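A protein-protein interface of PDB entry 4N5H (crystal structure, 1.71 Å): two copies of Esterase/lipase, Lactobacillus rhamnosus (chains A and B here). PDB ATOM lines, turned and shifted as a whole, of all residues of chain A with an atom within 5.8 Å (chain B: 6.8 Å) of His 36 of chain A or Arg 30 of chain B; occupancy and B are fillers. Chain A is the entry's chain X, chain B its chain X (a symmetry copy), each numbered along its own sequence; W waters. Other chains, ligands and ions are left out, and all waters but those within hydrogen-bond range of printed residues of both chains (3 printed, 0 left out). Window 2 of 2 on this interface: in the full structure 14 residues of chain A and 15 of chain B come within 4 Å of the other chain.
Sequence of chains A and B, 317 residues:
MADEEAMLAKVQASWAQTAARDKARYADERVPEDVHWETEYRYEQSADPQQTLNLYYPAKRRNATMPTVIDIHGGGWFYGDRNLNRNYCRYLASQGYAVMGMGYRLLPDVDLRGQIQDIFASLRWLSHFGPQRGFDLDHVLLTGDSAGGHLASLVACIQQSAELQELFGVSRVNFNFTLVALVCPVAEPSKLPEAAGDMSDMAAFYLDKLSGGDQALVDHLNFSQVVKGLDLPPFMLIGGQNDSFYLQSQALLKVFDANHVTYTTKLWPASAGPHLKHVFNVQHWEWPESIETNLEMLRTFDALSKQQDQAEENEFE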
ATOM      1  N   ASP A  34     -13.994 -36.347  22.586  1.00  0.00           N
ATOM      2  CA  ASP A  34     -12.982 -36.278  23.619  1.00  0.00           C
ATOM      3  C   ASP A  34     -11.551 -36.193  23.093  1.00  0.00           C
ATOM      4  O   ASP A  34     -10.634 -36.794  23.596  1.00  0.00           O
ATOM      5  CB  ASP A  34     -13.133 -37.411  24.595  1.00  0.00           C
ATOM      6  CG  ASP A  34     -14.568 -37.482  25.199  1.00  0.00           C
ATOM      7  OD1 ASP A  34     -15.132 -36.418  25.550  1.00  0.00           O
ATOM      8  OD2 ASP A  34     -15.062 -38.622  25.274  1.00  0.00           O
ATOM      9  N   VAL A  35     -11.434 -35.491  21.981  1.00  0.00           N
ATOM     10  CA  VAL A  35     -10.117 -35.229  21.345  1.00  0.00           C
ATOM     11  C   VAL A  35      -9.965 -33.727  21.073  1.00  0.00           C
ATOM     12  O   VAL A  35     -10.984 -33.041  20.811  1.00  0.00           O
ATOM     13  CB  VAL A  35     -10.053 -36.006  20.021  1.00  0.00           C
ATOM     14  CG1 VAL A  35      -8.819 -35.677  19.179  1.00  0.00           C
ATOM     15  CG2 VAL A  35     -10.053 -37.497  20.361  1.00  0.00           C
ATOM     16  N   HIS A  36      -8.728 -33.267  21.183  1.00  0.00           N
ATOM     17  CA  HIS A  36      -8.327 -31.907  20.787  1.00  0.00           C
ATOM     18  C   HIS A  36      -7.348 -32.031  19.603  1.00  0.00           C
ATOM     19  O   HIS A  36      -6.562 -32.924  19.540  1.00  0.00           O
ATOM     20  CB  HIS A  36      -7.582 -31.195  21.902  1.00  0.00           C
ATOM     21  CG  HIS A  36      -8.428 -30.865  23.096  1.00  0.00           C
ATOM     22  ND1 HIS A  36      -7.896 -30.506  24.313  1.00  0.00           N
ATOM     23  CD2 HIS A  36      -9.755 -30.828  23.234  1.00  0.00           C
ATOM     24  CE1 HIS A  36      -8.880 -30.287  25.170  1.00  0.00           C
ATOM     25  NE2 HIS A  36     -10.018 -30.474  24.536  1.00  0.00           N
ATOM     26  N   TRP A  37      -7.412 -31.063  18.718  1.00  0.00           N
ATOM     27  CA  TRP A  37      -6.462 -31.016  17.604  1.00  0.00           C
ATOM     28  C   TRP A  37      -5.857 -29.577  17.501  1.00  0.00           C
ATOM     29  O   TRP A  37      -6.526 -28.583  17.848  1.00  0.00           O
ATOM     30  CB  TRP A  37      -6.974 -31.524  16.244  1.00  0.00           C
ATOM     31  CG  TRP A  37      -7.981 -30.736  15.369  1.00  0.00           C
ATOM     32  CD1 TRP A  37      -8.817 -29.750  15.731  1.00  0.00           C
ATOM     33  CD2 TRP A  37      -8.300 -31.026  13.964  1.00  0.00           C
ATOM     34  NE1 TRP A  37      -9.611 -29.391  14.707  1.00  0.00           N
ATOM     35  CE2 TRP A  37      -9.338 -30.156  13.595  1.00  0.00           C
ATOM     36  CE3 TRP A  37      -7.817 -31.945  13.010  1.00  0.00           C
ATOM     37  CZ2 TRP A  37      -9.944 -30.209  12.295  1.00  0.00           C
ATOM     38  CZ3 TRP A  37      -8.324 -31.898  11.672  1.00  0.00           C
ATOM     39  CH2 TRP A  37      -9.381 -31.059  11.349  1.00  0.00           C
ATOM     40  N   GLU A  38      -4.650 -29.530  16.912  1.00  0.00           N
ATOM     41  CA  GLU A  38      -3.932 -28.338  16.611  1.00  0.00           C
ATOM     42  C   GLU A  38      -3.602 -28.463  15.111  1.00  0.00           C
ATOM     43  O   GLU A  38      -2.967 -29.409  14.709  1.00  0.00           O
ATOM     44  CB  GLU A  38      -2.631 -28.319  17.428  1.00  0.00           C
ATOM     45  CG  GLU A  38      -2.830 -28.213  18.937  1.00  0.00           C
ATOM     46  CD  GLU A  38      -1.607 -28.587  19.766  1.00  0.00           C
ATOM     47  OE1 GLU A  38      -0.552 -28.948  19.197  1.00  0.00           O
ATOM     48  OE2 GLU A  38      -1.719 -28.687  21.043  1.00  0.00           O
ATOM     49  N   THR A  39      -4.017 -27.478  14.353  1.00  0.00           N
ATOM     50  CA  THR A  39      -4.021 -27.652  12.909  1.00  0.00           C
ATOM     51  C   THR A  39      -3.046 -26.745  12.173  1.00  0.00           C
ATOM     52  O   THR A  39      -2.703 -25.644  12.667  1.00  0.00           O
ATOM     53  CB  THR A  39      -5.440 -27.451  12.329  1.00  0.00           C
ATOM     54  OG1 THR A  39      -5.949 -26.177  12.695  1.00  0.00           O
ATOM     55  CG2 THR A  39      -6.363 -28.526  12.816  1.00  0.00           C
ATOM     56  N   LEU A  55      -1.829 -32.078  14.500  1.00  0.00           N
ATOM     57  CA  LEU A  55      -1.576 -32.848  15.738  1.00  0.00           C
ATOM     58  C   LEU A  55      -2.888 -33.094  16.462  1.00  0.00           C
ATOM     59  O   LEU A  55      -3.748 -32.214  16.625  1.00  0.00           O
ATOM     60  CB  LEU A  55      -0.617 -32.138  16.676  1.00  0.00           C
ATOM     61  CG  LEU A  55       0.709 -31.649  16.023  1.00  0.00           C
ATOM     62  CD1 LEU A  55       1.571 -30.919  17.000  1.00  0.00           C
ATOM     63  CD2 LEU A  55       1.474 -32.819  15.416  1.00  0.00           C
ATOM     64  N   TYR A  56      -3.000 -34.303  17.040  1.00  0.00           N
ATOM     65  CA  TYR A  56      -4.241 -34.724  17.691  1.00  0.00           C
ATOM     66  C   TYR A  56      -3.861 -35.348  19.059  1.00  0.00           C
ATOM     67  O   TYR A  56      -2.835 -36.050  19.206  1.00  0.00           O
ATOM     68  CB  TYR A  56      -4.985 -35.812  16.905  1.00  0.00           C
ATOM     69  CG  TYR A  56      -5.195 -35.525  15.439  1.00  0.00           C
ATOM     70  CD1 TYR A  56      -4.204 -35.711  14.504  1.00  0.00           C
ATOM     71  CD2 TYR A  56      -6.465 -35.148  14.992  1.00  0.00           C
ATOM     72  CE1 TYR A  56      -4.419 -35.474  13.151  1.00  0.00           C
ATOM     73  CE2 TYR A  56      -6.705 -34.955  13.629  1.00  0.00           C
ATOM     74  CZ  TYR A  56      -5.646 -35.084  12.712  1.00  0.00           C
ATOM     75  OH  TYR A  56      -5.895 -34.931  11.361  1.00  0.00           O
ATOM     76  N   TYR A  57      -4.730 -35.131  20.041  1.00  0.00           N
ATOM     77  CA  TYR A  57      -4.507 -35.600  21.396  1.00  0.00           C
ATOM     78  C   TYR A  57      -5.847 -35.918  22.102  1.00  0.00           C
ATOM     79  O   TYR A  57      -6.877 -35.393  21.814  1.00  0.00           O
ATOM     80  CB  TYR A  57      -3.966 -34.400  22.235  1.00  0.00           C
ATOM     81  CG  TYR A  57      -2.784 -33.647  21.622  1.00  0.00           C
ATOM     82  CD1 TYR A  57      -3.006 -32.580  20.803  1.00  0.00           C
ATOM     83  CD2 TYR A  57      -1.485 -33.973  21.897  1.00  0.00           C
ATOM     84  CE1 TYR A  57      -2.004 -31.864  20.249  1.00  0.00           C
ATOM     85  CE2 TYR A  57      -0.437 -33.252  21.371  1.00  0.00           C
ATOM     86  CZ  TYR A  57      -0.715 -32.156  20.524  1.00  0.00           C
ATOM     87  OH  TYR A  57       0.331 -31.417  20.020  1.00  0.00           O
ATOM     88  N   PRO A  58      -5.735 -36.805  23.083  1.00  0.00           N
ATOM     89  CA  PRO A  58      -6.967 -36.963  23.932  1.00  0.00           C
ATOM     90  C   PRO A  58      -7.276 -35.658  24.610  1.00  0.00           C
ATOM     91  O   PRO A  58      -6.336 -34.917  24.913  1.00  0.00           O
ATOM     92  CB  PRO A  58      -6.482 -38.029  24.962  1.00  0.00           C
ATOM     93  CG  PRO A  58      -5.015 -38.009  24.918  1.00  0.00           C
ATOM     94  CD  PRO A  58      -4.574 -37.547  23.579  1.00  0.00           C
ATOM     95  N   ALA A  59      -8.549 -35.340  24.804  1.00  0.00           N
ATOM     96  CA  ALA A  59      -8.873 -34.128  25.530  1.00  0.00           C
ATOM     97  C   ALA A  59      -8.371 -34.094  26.958  1.00  0.00           C
ATOM     98  O   ALA A  59      -8.000 -33.022  27.382  1.00  0.00           O
ATOM     99  CB  ALA A  59     -10.353 -33.837  25.458  1.00  0.00           C
ATOM    100  N   LYS A  60      -8.346 -35.182  27.664  1.00  0.00           N
ATOM    101  CA  LYS A  60      -7.764 -35.191  29.012  1.00  0.00           C
ATOM    102  C   LYS A  60      -6.581 -36.097  28.973  1.00  0.00           C
ATOM    103  O   LYS A  60      -6.741 -37.287  28.722  1.00  0.00           O
ATOM    104  CB  LYS A  60      -8.852 -35.748  29.982  1.00  0.00           C
ATOM    105  N   ALA A  93      -5.990 -40.953  18.708  1.00  0.00           N
ATOM    106  CA  ALA A  93      -5.673 -40.016  19.802  1.00  0.00           C
ATOM    107  C   ALA A  93      -6.579 -40.219  21.021  1.00  0.00           C
ATOM    108  O   ALA A  93      -6.097 -40.157  22.162  1.00  0.00           O
ATOM    109  CB  ALA A  93      -5.802 -38.539  19.317  1.00  0.00           C
ATOM    110  N   ARG B  25      -9.202 -22.506   7.086  1.00  0.00           N
ATOM    111  CA  ARG B  25      -8.669 -22.612   8.503  1.00  0.00           C
ATOM    112  C   ARG B  25      -9.783 -22.611   9.493  1.00  0.00           C
ATOM    113  O   ARG B  25      -9.771 -23.446  10.443  1.00  0.00           O
ATOM    114  CB  ARG B  25      -7.694 -21.472   8.785  1.00  0.00           C
ATOM    115  CG  ARG B  25      -7.160 -21.509  10.228  1.00  0.00           C
ATOM    116  CD  ARG B  25      -6.302 -20.263  10.568  1.00  0.00           C
ATOM    117  NE  ARG B  25      -5.422 -20.051   9.469  1.00  0.00           N
ATOM    118  CZ  ARG B  25      -5.474 -19.033   8.600  1.00  0.00           C
ATOM    119  NH1 ARG B  25      -6.254 -18.041   8.833  1.00  0.00           N
ATOM    120  NH2 ARG B  25      -4.739 -19.077   7.519  1.00  0.00           N
ATOM    121  N   TYR B  26     -10.762 -21.670   9.432  1.00  0.00           N
ATOM    122  CA  TYR B  26     -11.812 -21.602  10.386  1.00  0.00           C
ATOM    123  C   TYR B  26     -12.754 -22.808  10.295  1.00  0.00           C
ATOM    124  O   TYR B  26     -13.347 -23.195  11.289  1.00  0.00           O
ATOM    125  CB  TYR B  26     -12.649 -20.404  10.129  1.00  0.00           C
ATOM    126  CG  TYR B  26     -12.161 -19.316  10.977  1.00  0.00           C
ATOM    127  CD1 TYR B  26     -12.634 -19.259  12.295  1.00  0.00           C
ATOM    128  CD2 TYR B  26     -11.343 -18.265  10.484  1.00  0.00           C
ATOM    129  CE1 TYR B  26     -12.233 -18.238  13.154  1.00  0.00           C
ATOM    130  CE2 TYR B  26     -10.972 -17.196  11.343  1.00  0.00           C
ATOM    131  CZ  TYR B  26     -11.399 -17.214  12.684  1.00  0.00           C
ATOM    132  OH  TYR B  26     -11.109 -16.288  13.649  1.00  0.00           O
ATOM    133  N   ASP B  28     -11.844 -25.774  10.055  1.00  0.00           N
ATOM    134  CA  ASP B  28     -11.330 -26.866  10.803  1.00  0.00           C
ATOM    135  C   ASP B  28     -10.911 -26.607  12.276  1.00  0.00           C
ATOM    136  O   ASP B  28     -10.889 -27.490  13.101  1.00  0.00           O
ATOM    137  CB  ASP B  28     -10.126 -27.324  10.128  1.00  0.00           C
ATOM    138  CG  ASP B  28     -10.431 -28.065   8.817  1.00  0.00           C
ATOM    139  OD1 ASP B  28     -11.506 -28.648   8.647  1.00  0.00           O
ATOM    140  OD2 ASP B  28      -9.584 -27.984   7.971  1.00  0.00           O
ATOM    141  N   GLU B  29     -10.512 -25.390  12.540  1.00  0.00           N
ATOM    142  CA  GLU B  29      -9.865 -25.072  13.784  1.00  0.00           C
ATOM    143  C   GLU B  29     -10.783 -25.283  14.949  1.00  0.00           C
ATOM    144  O   GLU B  29     -11.997 -24.889  14.925  1.00  0.00           O
ATOM    145  CB  GLU B  29      -9.391 -23.609  13.716  1.00  0.00           C
ATOM    146  CG  GLU B  29      -8.467 -23.238  14.853  1.00  0.00           C
ATOM    147  CD  GLU B  29      -8.161 -21.757  15.012  1.00  0.00           C
ATOM    148  OE1 GLU B  29      -8.801 -20.851  14.420  1.00  0.00           O
ATOM    149  OE2 GLU B  29      -7.233 -21.484  15.803  1.00  0.00           O
ATOM    150  N   ARG B  30     -10.217 -25.807  16.046  1.00  0.00           N
ATOM    151  CA  ARG B  30     -10.900 -25.806  17.317  1.00  0.00           C
ATOM    152  C   ARG B  30     -11.355 -24.417  17.713  1.00  0.00           C
ATOM    153  O   ARG B  30     -10.605 -23.439  17.554  1.00  0.00           O
ATOM    154  CB  ARG B  30      -9.954 -26.304  18.405  1.00  0.00           C
ATOM    155  CG  ARG B  30     -10.620 -26.599  19.752  1.00  0.00           C
ATOM    156  CD  ARG B  30      -9.563 -27.089  20.708  1.00  0.00           C
ATOM    157  NE  ARG B  30     -10.051 -27.020  22.071  1.00  0.00           N
ATOM    158  CZ  ARG B  30      -9.276 -27.033  23.109  1.00  0.00           C
ATOM    159  NH1 ARG B  30      -7.968 -27.232  22.965  1.00  0.00           N
ATOM    160  NH2 ARG B  30      -9.830 -26.916  24.347  1.00  0.00           N
ATOM    161  N   VAL B  31     -12.550 -24.319  18.256  1.00  0.00           N
ATOM    162  CA  VAL B  31     -13.061 -23.012  18.763  1.00  0.00           C
ATOM    163  C   VAL B  31     -12.931 -22.938  20.256  1.00  0.00           C
ATOM    164  O   VAL B  31     -13.284 -23.894  20.934  1.00  0.00           O
ATOM    165  CB  VAL B  31     -14.521 -22.890  18.375  1.00  0.00           C
ATOM    166  CG1 VAL B  31     -15.106 -21.647  18.902  1.00  0.00           C
ATOM    167  CG2 VAL B  31     -14.700 -22.978  16.862  1.00  0.00           C
ATOM    168  N   PRO B  32     -12.517 -21.768  20.804  1.00  0.00           N
ATOM    169  CA  PRO B  32     -12.400 -21.707  22.248  1.00  0.00           C
ATOM    170  C   PRO B  32     -13.777 -21.901  22.892  1.00  0.00           C
ATOM    171  O   PRO B  32     -14.712 -21.324  22.423  1.00  0.00           O
ATOM    172  CB  PRO B  32     -11.778 -20.297  22.507  1.00  0.00           C
ATOM    173  CG  PRO B  32     -11.174 -19.947  21.244  1.00  0.00           C
ATOM    174  CD  PRO B  32     -11.950 -20.580  20.138  1.00  0.00           C
ATOM    175  N   GLU B  33     -13.826 -22.689  23.925  1.00  0.00           N
ATOM    176  CA  GLU B  33     -15.091 -22.987  24.588  1.00  0.00           C
ATOM    177  C   GLU B  33     -15.352 -21.963  25.757  1.00  0.00           C
ATOM    178  O   GLU B  33     -14.486 -21.171  26.214  1.00  0.00           O
ATOM    179  CB  GLU B  33     -15.024 -24.379  25.272  1.00  0.00           C
ATOM    180  CG  GLU B  33     -14.622 -25.572  24.395  1.00  0.00           C
ATOM    181  CD  GLU B  33     -14.044 -26.752  25.197  1.00  0.00           C
ATOM    182  OE1 GLU B  33     -12.796 -26.839  25.351  1.00  0.00           O
ATOM    183  OE2 GLU B  33     -14.837 -27.589  25.688  1.00  0.00           O
ATOM    184  N   ASN B  87     -11.757 -16.216  16.609  1.00  0.00           N
ATOM    185  CA  ASN B  87     -11.255 -17.274  17.517  1.00  0.00           C
ATOM    186  C   ASN B  87     -10.225 -16.694  18.483  1.00  0.00           C
ATOM    187  O   ASN B  87     -10.271 -17.021  19.646  1.00  0.00           O
ATOM    188  CB  ASN B  87     -10.666 -18.435  16.746  1.00  0.00           C
ATOM    189  CG  ASN B  87     -11.784 -19.372  16.252  1.00  0.00           C
ATOM    190  OD1 ASN B  87     -13.014 -19.195  16.556  1.00  0.00           O
ATOM    191  ND2 ASN B  87     -11.378 -20.359  15.498  1.00  0.00           N
ATOM    192  N   TRP B 285      -4.934 -19.892  17.856  1.00  0.00           N
ATOM    193  CA  TRP B 285      -4.930 -19.729  19.317  1.00  0.00           C
ATOM    194  C   TRP B 285      -4.552 -20.964  20.069  1.00  0.00           C
ATOM    195  O   TRP B 285      -4.017 -20.876  21.166  1.00  0.00           O
ATOM    196  CB  TRP B 285      -6.318 -19.252  19.771  1.00  0.00           C
ATOM    197  CG  TRP B 285      -7.347 -20.314  19.725  1.00  0.00           C
ATOM    198  CD1 TRP B 285      -8.095 -20.679  18.660  1.00  0.00           C
ATOM    199  CD2 TRP B 285      -7.617 -21.283  20.752  1.00  0.00           C
ATOM    200  NE1 TRP B 285      -8.833 -21.814  18.985  1.00  0.00           N
ATOM    201  CE2 TRP B 285      -8.612 -22.147  20.269  1.00  0.00           C
ATOM    202  CE3 TRP B 285      -7.214 -21.414  22.076  1.00  0.00           C
ATOM    203  CZ2 TRP B 285      -9.127 -23.167  21.007  1.00  0.00           C
ATOM    204  CZ3 TRP B 285      -7.669 -22.437  22.776  1.00  0.00           C
ATOM    205  CH2 TRP B 285      -8.634 -23.326  22.279  1.00  0.00           C
ATOM    206  N   GLU B 286      -4.820 -22.134  19.445  1.00  0.00           N
ATOM    207  CA  GLU B 286      -4.766 -23.388  20.184  1.00  0.00           C
ATOM    208  C   GLU B 286      -3.333 -23.945  20.258  1.00  0.00           C
ATOM    209  O   GLU B 286      -3.064 -24.869  20.999  1.00  0.00           O
ATOM    210  CB  GLU B 286      -5.756 -24.386  19.507  1.00  0.00           C
ATOM    211  CG  GLU B 286      -5.291 -25.100  18.228  1.00  0.00           C
ATOM    212  CD  GLU B 286      -5.360 -24.292  16.945  1.00  0.00           C
ATOM    213  OE1 GLU B 286      -5.627 -23.052  16.986  1.00  0.00           O
ATOM    214  OE2 GLU B 286      -5.118 -24.857  15.890  1.00  0.00           O
HETATM  215  O   HOH W   1      -6.394 -28.032  20.654  1.00  0.00           O
HETATM  216  O   HOH W   2      -7.469 -26.680  15.931  1.00  0.00           O
HETATM  217  O   HOH W   3      -7.419 -25.166  10.749  1.00  0.00           O
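Water W3 bridges the side-chain hydroxyl of Thr 39 of chain A (2.6 Å) and the backbone carbonyl oxygen of Arg 25 of chain B (2.9 Å).
Water W2 lies within hydrogen-bond range of the backbone carbonyl oxygen of Trp 37 of chain A (2.9 Å), the backbone NH of Arg 30 of chain B (2.9 Å) and the side-chain carboxylate of Glu 286 of chain B (3.0 Å).
Water W1 bridges O of Trp 37 of chain A and NH1 of Arg 30 of chain B.
N of His 36 of chain A lies within hydrogen-bond range of O of Tyr 57 of chain A (2.9 Å).
The backbone NH of Glu 38 of chain A is in hydrogen-bond range of the backbone carbonyl oxygen of Leu 55 of chain A (2.8 Å).
The side-chain carboxylate of Glu 38 of chain A sits at hydrogen-bond distance from the side-chain hydroxyl of Tyr 57 of chain A.
The side-chain carboxylate of Glu 29 of chain B sits close to the side-chain carboxylate of Glu 286 of chain B (2.5 Å).
The guanidinium group (NH2) of Arg 30 of chain B lies within salt-bridge range of the side-chain carboxylate (OE1) of Glu 33 of chain B (3.1 Å).
The backbone carbonyl oxygen (O) of Arg 30 of chain B lies within hydrogen-bond range of the indole nitrogen (NE1) of Trp 285 of chain B.
ND1 of His 36 of chain A touches NH1 of Arg 30 of chain B, 3.5 Å away.
Arg 30 of chain B touches Trp 37 of chain A (N to NE1, 3.9 Å).
Trp 37 of chain A touches Glu 286 of chain B.
Glu 38 of chain A touches Glu 286 of chain B (CA to OE2, 3.7 Å).
Of chain B, only Arg 30 comes within 4 Å of His 36 of chain A.
Of the printed residues of chain B, Trp 37 of chain A touches Asp 28 (2.8 Å), Arg 30 (3.9 Å) and Glu 286 (3.7 Å).
Of the printed residues of chain B, Glu 38 of chain A touches Glu 286 (3.7 Å).
Of the printed residues of chain B, Thr 39 of chain A touches Glu 286 (3.2 Å).
Of the printed residues of chain A, Arg 30 of chain B touches His 36 and Trp 37.
Of the printed residues of chain A, Glu 286 of chain B touches Trp 37, Glu 38 and Thr 39.
The nearest residue of chain B that does not touch His 36 of chain A is Glu 33 of chain B (4.6 Å).
The nearest printed residue of chain B that does not touch Glu 38 of chain A is Arg 30 of chain B (6.4 Å).
No position is printed for both chains.
Of the 6 pairs that touch across the chains among the printed residues, none has its exchanged pair printed and touching as well.
O of Asp 28 of chain B is in hydrogen-bond range of NE1 of Trp 37 of chain A (2.8 Å).
N of Thr 39 of chain A sits at hydrogen-bond distance from OE2 of Glu 286 of chain B.
Printed residues of chain A that touch a printed residue of chain B: His 36, Trp 37, Glu 38 and Thr 39.
Hydrophobic or aromatic side chains of chain A that line the printed part of chain B: His 36 and Trp 37.
Of the 11 printed residues of chain B, 3 touch a printed residue of chain A.
Printed residues of chain B that touch a printed residue of chain A: Asp 28, Arg 30 and Glu 286.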
